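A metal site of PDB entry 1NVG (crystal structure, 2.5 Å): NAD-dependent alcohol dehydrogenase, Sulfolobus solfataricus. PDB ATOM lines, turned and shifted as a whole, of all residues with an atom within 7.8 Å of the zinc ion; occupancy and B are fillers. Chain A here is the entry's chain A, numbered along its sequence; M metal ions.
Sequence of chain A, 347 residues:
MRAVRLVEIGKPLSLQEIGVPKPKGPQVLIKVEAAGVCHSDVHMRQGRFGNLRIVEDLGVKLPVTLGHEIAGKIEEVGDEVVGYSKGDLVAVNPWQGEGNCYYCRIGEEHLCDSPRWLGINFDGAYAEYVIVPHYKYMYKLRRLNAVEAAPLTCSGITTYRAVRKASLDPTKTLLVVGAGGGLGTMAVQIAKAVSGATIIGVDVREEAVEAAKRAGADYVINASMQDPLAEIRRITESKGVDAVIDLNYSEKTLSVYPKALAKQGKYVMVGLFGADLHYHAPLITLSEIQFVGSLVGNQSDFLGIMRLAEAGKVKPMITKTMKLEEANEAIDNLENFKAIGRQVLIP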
ATOM      1  N   GLY A  36     -19.308  17.049 -24.199  1.00  0.00           N
ATOM      2  CA  GLY A  36     -19.777  15.921 -23.411  1.00  0.00           C
ATOM      3  C   GLY A  36     -18.875  14.694 -23.471  1.00  0.00           C
ATOM      4  O   GLY A  36     -18.153  14.468 -24.455  1.00  0.00           O
ATOM      5  N   VAL A  37     -18.922  13.908 -22.409  1.00  0.00           N
ATOM      6  CA  VAL A  37     -18.142  12.680 -22.328  1.00  0.00           C
ATOM      7  C   VAL A  37     -19.121  11.577 -21.935  1.00  0.00           C
ATOM      8  O   VAL A  37     -19.877  11.748 -20.980  1.00  0.00           O
ATOM      9  CB  VAL A  37     -17.062  12.799 -21.226  1.00  0.00           C
ATOM     10  CG1 VAL A  37     -16.197  11.553 -21.186  1.00  0.00           C
ATOM     11  CG2 VAL A  37     -16.218  14.046 -21.468  1.00  0.00           C
ATOM     12  N   CYS A  38     -19.145  10.480 -22.674  1.00  0.00           N
ATOM     13  CA  CYS A  38     -20.028   9.349 -22.339  1.00  0.00           C
ATOM     14  C   CYS A  38     -19.230   8.046 -22.387  1.00  0.00           C
ATOM     15  O   CYS A  38     -18.069   8.049 -22.813  1.00  0.00           O
ATOM     16  CB  CYS A  38     -21.249   9.268 -23.277  1.00  0.00           C
ATOM     17  SG  CYS A  38     -20.957   8.640 -24.962  1.00  0.00           S
ATOM     18  N   HIS A  39     -19.857   6.952 -21.952  1.00  0.00           N
ATOM     19  CA  HIS A  39     -19.175   5.669 -21.881  1.00  0.00           C
ATOM     20  C   HIS A  39     -18.502   5.311 -23.207  1.00  0.00           C
ATOM     21  O   HIS A  39     -17.488   4.617 -23.227  1.00  0.00           O
ATOM     22  CB  HIS A  39     -20.151   4.549 -21.455  1.00  0.00           C
ATOM     23  CG  HIS A  39     -19.485   3.374 -20.813  1.00  0.00           C
ATOM     24  ND1 HIS A  39     -18.810   3.460 -19.606  1.00  0.00           N
ATOM     25  CD2 HIS A  39     -19.379   2.082 -21.204  1.00  0.00           C
ATOM     26  CE1 HIS A  39     -18.312   2.277 -19.294  1.00  0.00           C
ATOM     27  NE2 HIS A  39     -18.641   1.424 -20.250  1.00  0.00           N
ATOM     28  N   SER A  40     -19.065   5.815 -24.314  1.00  0.00           N
ATOM     29  CA  SER A  40     -18.489   5.578 -25.647  1.00  0.00           C
ATOM     30  C   SER A  40     -17.017   5.953 -25.640  1.00  0.00           C
ATOM     31  O   SER A  40     -16.200   5.315 -26.304  1.00  0.00           O
ATOM     32  CB  SER A  40     -19.188   6.426 -26.705  1.00  0.00           C
ATOM     33  OG  SER A  40     -20.596   6.260 -26.687  1.00  0.00           O
ATOM     34  N   ASP A  41     -16.677   6.996 -24.882  1.00  0.00           N
ATOM     35  CA  ASP A  41     -15.309   7.486 -24.832  1.00  0.00           C
ATOM     36  C   ASP A  41     -14.360   6.538 -24.115  1.00  0.00           C
ATOM     37  O   ASP A  41     -13.154   6.621 -24.295  1.00  0.00           O
ATOM     38  CB  ASP A  41     -15.255   8.869 -24.195  1.00  0.00           C
ATOM     39  CG  ASP A  41     -15.761   9.950 -25.117  1.00  0.00           C
ATOM     40  OD1 ASP A  41     -15.329   9.959 -26.288  1.00  0.00           O
ATOM     41  OD2 ASP A  41     -16.581  10.782 -24.690  1.00  0.00           O
ATOM     42  N   PHE A  49     -14.736   0.958 -31.104  1.00  0.00           N
ATOM     43  CA  PHE A  49     -16.016   1.640 -31.016  1.00  0.00           C
ATOM     44  C   PHE A  49     -17.054   0.534 -31.074  1.00  0.00           C
ATOM     45  O   PHE A  49     -17.707   0.334 -32.100  1.00  0.00           O
ATOM     46  CB  PHE A  49     -16.237   2.606 -32.187  1.00  0.00           C
ATOM     47  CG  PHE A  49     -17.527   3.376 -32.091  1.00  0.00           C
ATOM     48  CD1 PHE A  49     -17.645   4.456 -31.225  1.00  0.00           C
ATOM     49  CD2 PHE A  49     -18.656   2.979 -32.810  1.00  0.00           C
ATOM     50  CE1 PHE A  49     -18.861   5.141 -31.088  1.00  0.00           C
ATOM     51  CE2 PHE A  49     -19.871   3.659 -32.681  1.00  0.00           C
ATOM     52  CZ  PHE A  49     -19.980   4.738 -31.814  1.00  0.00           C
ATOM     53  N   GLY A  67     -14.357  13.704 -28.646  1.00  0.00           N
ATOM     54  CA  GLY A  67     -15.412  14.664 -28.388  1.00  0.00           C
ATOM     55  C   GLY A  67     -16.476  14.688 -29.478  1.00  0.00           C
ATOM     56  O   GLY A  67     -16.394  15.488 -30.418  1.00  0.00           O
ATOM     57  N   HIS A  68     -17.470  13.818 -29.344  1.00  0.00           N
ATOM     58  CA  HIS A  68     -18.544  13.734 -30.316  1.00  0.00           C
ATOM     59  C   HIS A  68     -19.793  14.409 -29.807  1.00  0.00           C
ATOM     60  O   HIS A  68     -20.823  14.372 -30.469  1.00  0.00           O
ATOM     61  CB  HIS A  68     -18.854  12.283 -30.645  1.00  0.00           C
ATOM     62  CG  HIS A  68     -19.230  11.469 -29.441  1.00  0.00           C
ATOM     63  ND1 HIS A  68     -18.327  10.805 -28.646  1.00  0.00           N
ATOM     64  CD2 HIS A  68     -20.445  11.284 -28.859  1.00  0.00           C
ATOM     65  CE1 HIS A  68     -19.001  10.254 -27.623  1.00  0.00           C
ATOM     66  NE2 HIS A  68     -20.287  10.529 -27.707  1.00  0.00           N
ATOM     67  N   GLU A  69     -19.718  15.029 -28.633  1.00  0.00           N
ATOM     68  CA  GLU A  69     -20.869  15.738 -28.068  1.00  0.00           C
ATOM     69  C   GLU A  69     -20.532  17.225 -28.044  1.00  0.00           C
ATOM     70  O   GLU A  69     -19.835  17.702 -27.148  1.00  0.00           O
ATOM     71  CB  GLU A  69     -21.149  15.213 -26.640  1.00  0.00           C
ATOM     72  CG  GLU A  69     -21.300  13.696 -26.565  1.00  0.00           C
ATOM     73  CD  GLU A  69     -22.022  13.196 -25.298  1.00  0.00           C
ATOM     74  OE1 GLU A  69     -22.237  14.004 -24.353  1.00  0.00           O
ATOM     75  OE2 GLU A  69     -22.357  11.988 -25.237  1.00  0.00           O
ATOM     76  N   PRO A  94     -22.944  15.233 -34.982  1.00  0.00           N
ATOM     77  CA  PRO A  94     -21.672  14.627 -35.378  1.00  0.00           C
ATOM     78  C   PRO A  94     -21.744  13.390 -36.261  1.00  0.00           C
ATOM     79  O   PRO A  94     -20.700  12.901 -36.740  1.00  0.00           O
ATOM     80  CB  PRO A  94     -21.040  14.304 -34.024  1.00  0.00           C
ATOM     81  CG  PRO A  94     -22.231  13.803 -33.249  1.00  0.00           C
ATOM     82  CD  PRO A  94     -23.301  14.847 -33.604  1.00  0.00           C
ATOM     83  N   TRP A  95     -22.948  12.877 -36.482  1.00  0.00           N
ATOM     84  CA  TRP A  95     -23.112  11.631 -37.228  1.00  0.00           C
ATOM     85  C   TRP A  95     -23.353  11.934 -38.705  1.00  0.00           C
ATOM     86  O   TRP A  95     -24.447  11.725 -39.216  1.00  0.00           O
ATOM     87  CB  TRP A  95     -24.285  10.827 -36.638  1.00  0.00           C
ATOM     88  CG  TRP A  95     -24.291  10.855 -35.135  1.00  0.00           C
ATOM     89  CD1 TRP A  95     -25.151  11.553 -34.336  1.00  0.00           C
ATOM     90  CD2 TRP A  95     -23.330  10.254 -34.268  1.00  0.00           C
ATOM     91  NE1 TRP A  95     -24.773  11.433 -33.022  1.00  0.00           N
ATOM     92  CE2 TRP A  95     -23.651  10.638 -32.954  1.00  0.00           C
ATOM     93  CE3 TRP A  95     -22.215   9.428 -34.470  1.00  0.00           C
ATOM     94  CZ2 TRP A  95     -22.904  10.228 -31.841  1.00  0.00           C
ATOM     95  CZ3 TRP A  95     -21.466   9.021 -33.371  1.00  0.00           C
ATOM     96  CH2 TRP A  95     -21.815   9.417 -32.066  1.00  0.00           C
ATOM     97  N   ILE A 120     -14.881  10.804 -33.350  1.00  0.00           N
ATOM     98  CA  ILE A 120     -14.628   9.381 -33.461  1.00  0.00           C
ATOM     99  C   ILE A 120     -13.653   9.058 -34.591  1.00  0.00           C
ATOM    100  O   ILE A 120     -12.663   8.362 -34.369  1.00  0.00           O
ATOM    101  CB  ILE A 120     -15.966   8.632 -33.592  1.00  0.00           C
ATOM    102  CG1 ILE A 120     -16.759   8.873 -32.311  1.00  0.00           C
ATOM    103  CG2 ILE A 120     -15.752   7.139 -33.781  1.00  0.00           C
ATOM    104  CD1 ILE A 120     -18.106   8.331 -32.342  1.00  0.00           C
ATOM    105  N   ALA A 150     -25.185  20.077 -25.414  1.00  0.00           N
ATOM    106  CA  ALA A 150     -24.159  19.154 -25.868  1.00  0.00           C
ATOM    107  C   ALA A 150     -24.502  17.661 -25.716  1.00  0.00           C
ATOM    108  O   ALA A 150     -24.307  16.884 -26.633  1.00  0.00           O
ATOM    109  CB  ALA A 150     -22.830  19.477 -25.186  1.00  0.00           C
ATOM    110  N   PRO A 151     -24.996  17.249 -24.540  1.00  0.00           N
ATOM    111  CA  PRO A 151     -25.331  15.828 -24.382  1.00  0.00           C
ATOM    112  C   PRO A 151     -26.439  15.335 -25.332  1.00  0.00           C
ATOM    113  O   PRO A 151     -26.472  14.170 -25.712  1.00  0.00           O
ATOM    114  CB  PRO A 151     -25.735  15.736 -22.909  1.00  0.00           C
ATOM    115  CG  PRO A 151     -24.924  16.826 -22.270  1.00  0.00           C
ATOM    116  CD  PRO A 151     -25.089  17.954 -23.253  1.00  0.00           C
ATOM    117  N   THR A 153     -26.757  15.791 -28.351  1.00  0.00           N
ATOM    118  CA  THR A 153     -26.287  15.437 -29.683  1.00  0.00           C
ATOM    119  C   THR A 153     -25.948  13.959 -29.733  1.00  0.00           C
ATOM    120  O   THR A 153     -25.531  13.429 -30.774  1.00  0.00           O
ATOM    121  CB  THR A 153     -25.038  16.269 -30.065  1.00  0.00           C
ATOM    122  OG1 THR A 153     -23.941  15.902 -29.228  1.00  0.00           O
ATOM    123  CG2 THR A 153     -25.333  17.740 -29.904  1.00  0.00           C
ATOM    124  N   CYS A 154     -26.113  13.287 -28.594  1.00  0.00           N
ATOM    125  CA  CYS A 154     -25.757  11.880 -28.488  1.00  0.00           C
ATOM    126  C   CYS A 154     -26.819  11.063 -27.756  1.00  0.00           C
ATOM    127  O   CYS A 154     -27.438  10.185 -28.339  1.00  0.00           O
ATOM    128  CB  CYS A 154     -24.410  11.724 -27.787  1.00  0.00           C
ATOM    129  SG  CYS A 154     -23.799  10.023 -27.658  1.00  0.00           S
ATOM    130  N   SER A 155     -27.023  11.366 -26.480  1.00  0.00           N
ATOM    131  CA  SER A 155     -28.020  10.651 -25.686  1.00  0.00           C
ATOM    132  C   SER A 155     -29.386  11.104 -26.130  1.00  0.00           C
ATOM    133  O   SER A 155     -30.336  10.321 -26.157  1.00  0.00           O
ATOM    134  CB  SER A 155     -27.846  10.957 -24.201  1.00  0.00           C
ATOM    135  OG  SER A 155     -26.597  10.493 -23.736  1.00  0.00           O
ATOM    136  N   THR A 158     -30.078   9.617 -29.677  1.00  0.00           N
ATOM    137  CA  THR A 158     -30.116   8.173 -29.555  1.00  0.00           C
ATOM    138  C   THR A 158     -31.433   7.654 -28.986  1.00  0.00           C
ATOM    139  O   THR A 158     -32.039   6.739 -29.547  1.00  0.00           O
ATOM    140  CB  THR A 158     -28.962   7.674 -28.662  1.00  0.00           C
ATOM    141  OG1 THR A 158     -27.729   7.747 -29.399  1.00  0.00           O
ATOM    142  CG2 THR A 158     -29.175   6.242 -28.225  1.00  0.00           C
ATOM    143  N   LEU A 183     -29.696   7.888 -19.572  1.00  0.00           N
ATOM    144  CA  LEU A 183     -30.346   7.540 -20.825  1.00  0.00           C
ATOM    145  C   LEU A 183     -31.807   7.209 -20.580  1.00  0.00           C
ATOM    146  O   LEU A 183     -32.704   7.746 -21.245  1.00  0.00           O
ATOM    147  CB  LEU A 183     -29.646   6.328 -21.460  1.00  0.00           C
ATOM    148  CG  LEU A 183     -28.676   6.478 -22.639  1.00  0.00           C
ATOM    149  CD1 LEU A 183     -28.397   7.933 -22.946  1.00  0.00           C
ATOM    150  CD2 LEU A 183     -27.380   5.746 -22.307  1.00  0.00           C
ATOM    151  N   VAL A 296     -27.337   5.929 -32.556  1.00  0.00           N
ATOM    152  CA  VAL A 296     -27.413   7.360 -32.829  1.00  0.00           C
ATOM    153  C   VAL A 296     -28.680   7.715 -33.625  1.00  0.00           C
ATOM    154  O   VAL A 296     -29.773   7.294 -33.257  1.00  0.00           O
ATOM    155  CB  VAL A 296     -26.099   7.861 -33.537  1.00  0.00           C
ATOM    156  CG1 VAL A 296     -24.913   7.657 -32.602  1.00  0.00           C
ATOM    157  CG2 VAL A 296     -25.849   7.100 -34.827  1.00  0.00           C
ATOM    158  N   ARG A 342     -23.971  13.427 -16.313  1.00  0.00           N
ATOM    159  CA  ARG A 342     -23.217  13.481 -17.557  1.00  0.00           C
ATOM    160  C   ARG A 342     -22.094  14.508 -17.379  1.00  0.00           C
ATOM    161  O   ARG A 342     -22.348  15.673 -17.065  1.00  0.00           O
ATOM    162  CB  ARG A 342     -24.144  13.868 -18.715  1.00  0.00           C
ATOM    163  CG  ARG A 342     -23.424  14.127 -20.042  1.00  0.00           C
ATOM    164  CD  ARG A 342     -22.570  12.944 -20.441  1.00  0.00           C
ATOM    165  NE  ARG A 342     -23.365  11.736 -20.655  1.00  0.00           N
ATOM    166  CZ  ARG A 342     -24.086  11.494 -21.743  1.00  0.00           C
ATOM    167  NH1 ARG A 342     -24.130  12.357 -22.740  1.00  0.00           N
ATOM    168  NH2 ARG A 342     -24.768  10.357 -21.828  1.00  0.00           N
HETATM  169 ZN    ZN M   1     -21.869  10.298 -26.377  1.00  0.00          ZN
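The backbone carbonyl oxygen of Cys 154 is in hydrogen-bond range of the side-chain hydroxyl of Thr 158, at 2.7 Å. SG of Cys 38 sits close to OG of Ser 40 (3.0 Å). The side-chain carboxylate (OE1) of Glu 69 lies within salt-bridge range of the guanidinium group (NH1) of Arg 342 (3.0 Å). The backbone carbonyl oxygen of Glu 69 lies within hydrogen-bond range of the backbone NH of Gly 36, 3.1 Å away. N of Cys 38 lies within hydrogen-bond range of OD2 of Asp 41 (3.3 Å).
A ring nitrogen (NE2) of His 68 is bound to the zinc ion. The side-chain carboxylate (OE2) of Glu 69 binds the zinc ion (2.1 Å). The zinc ion is bound by SG of Cys 154, 2.3 Å away. The zinc ion is bound by SG of Cys 38 (2.4 Å).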
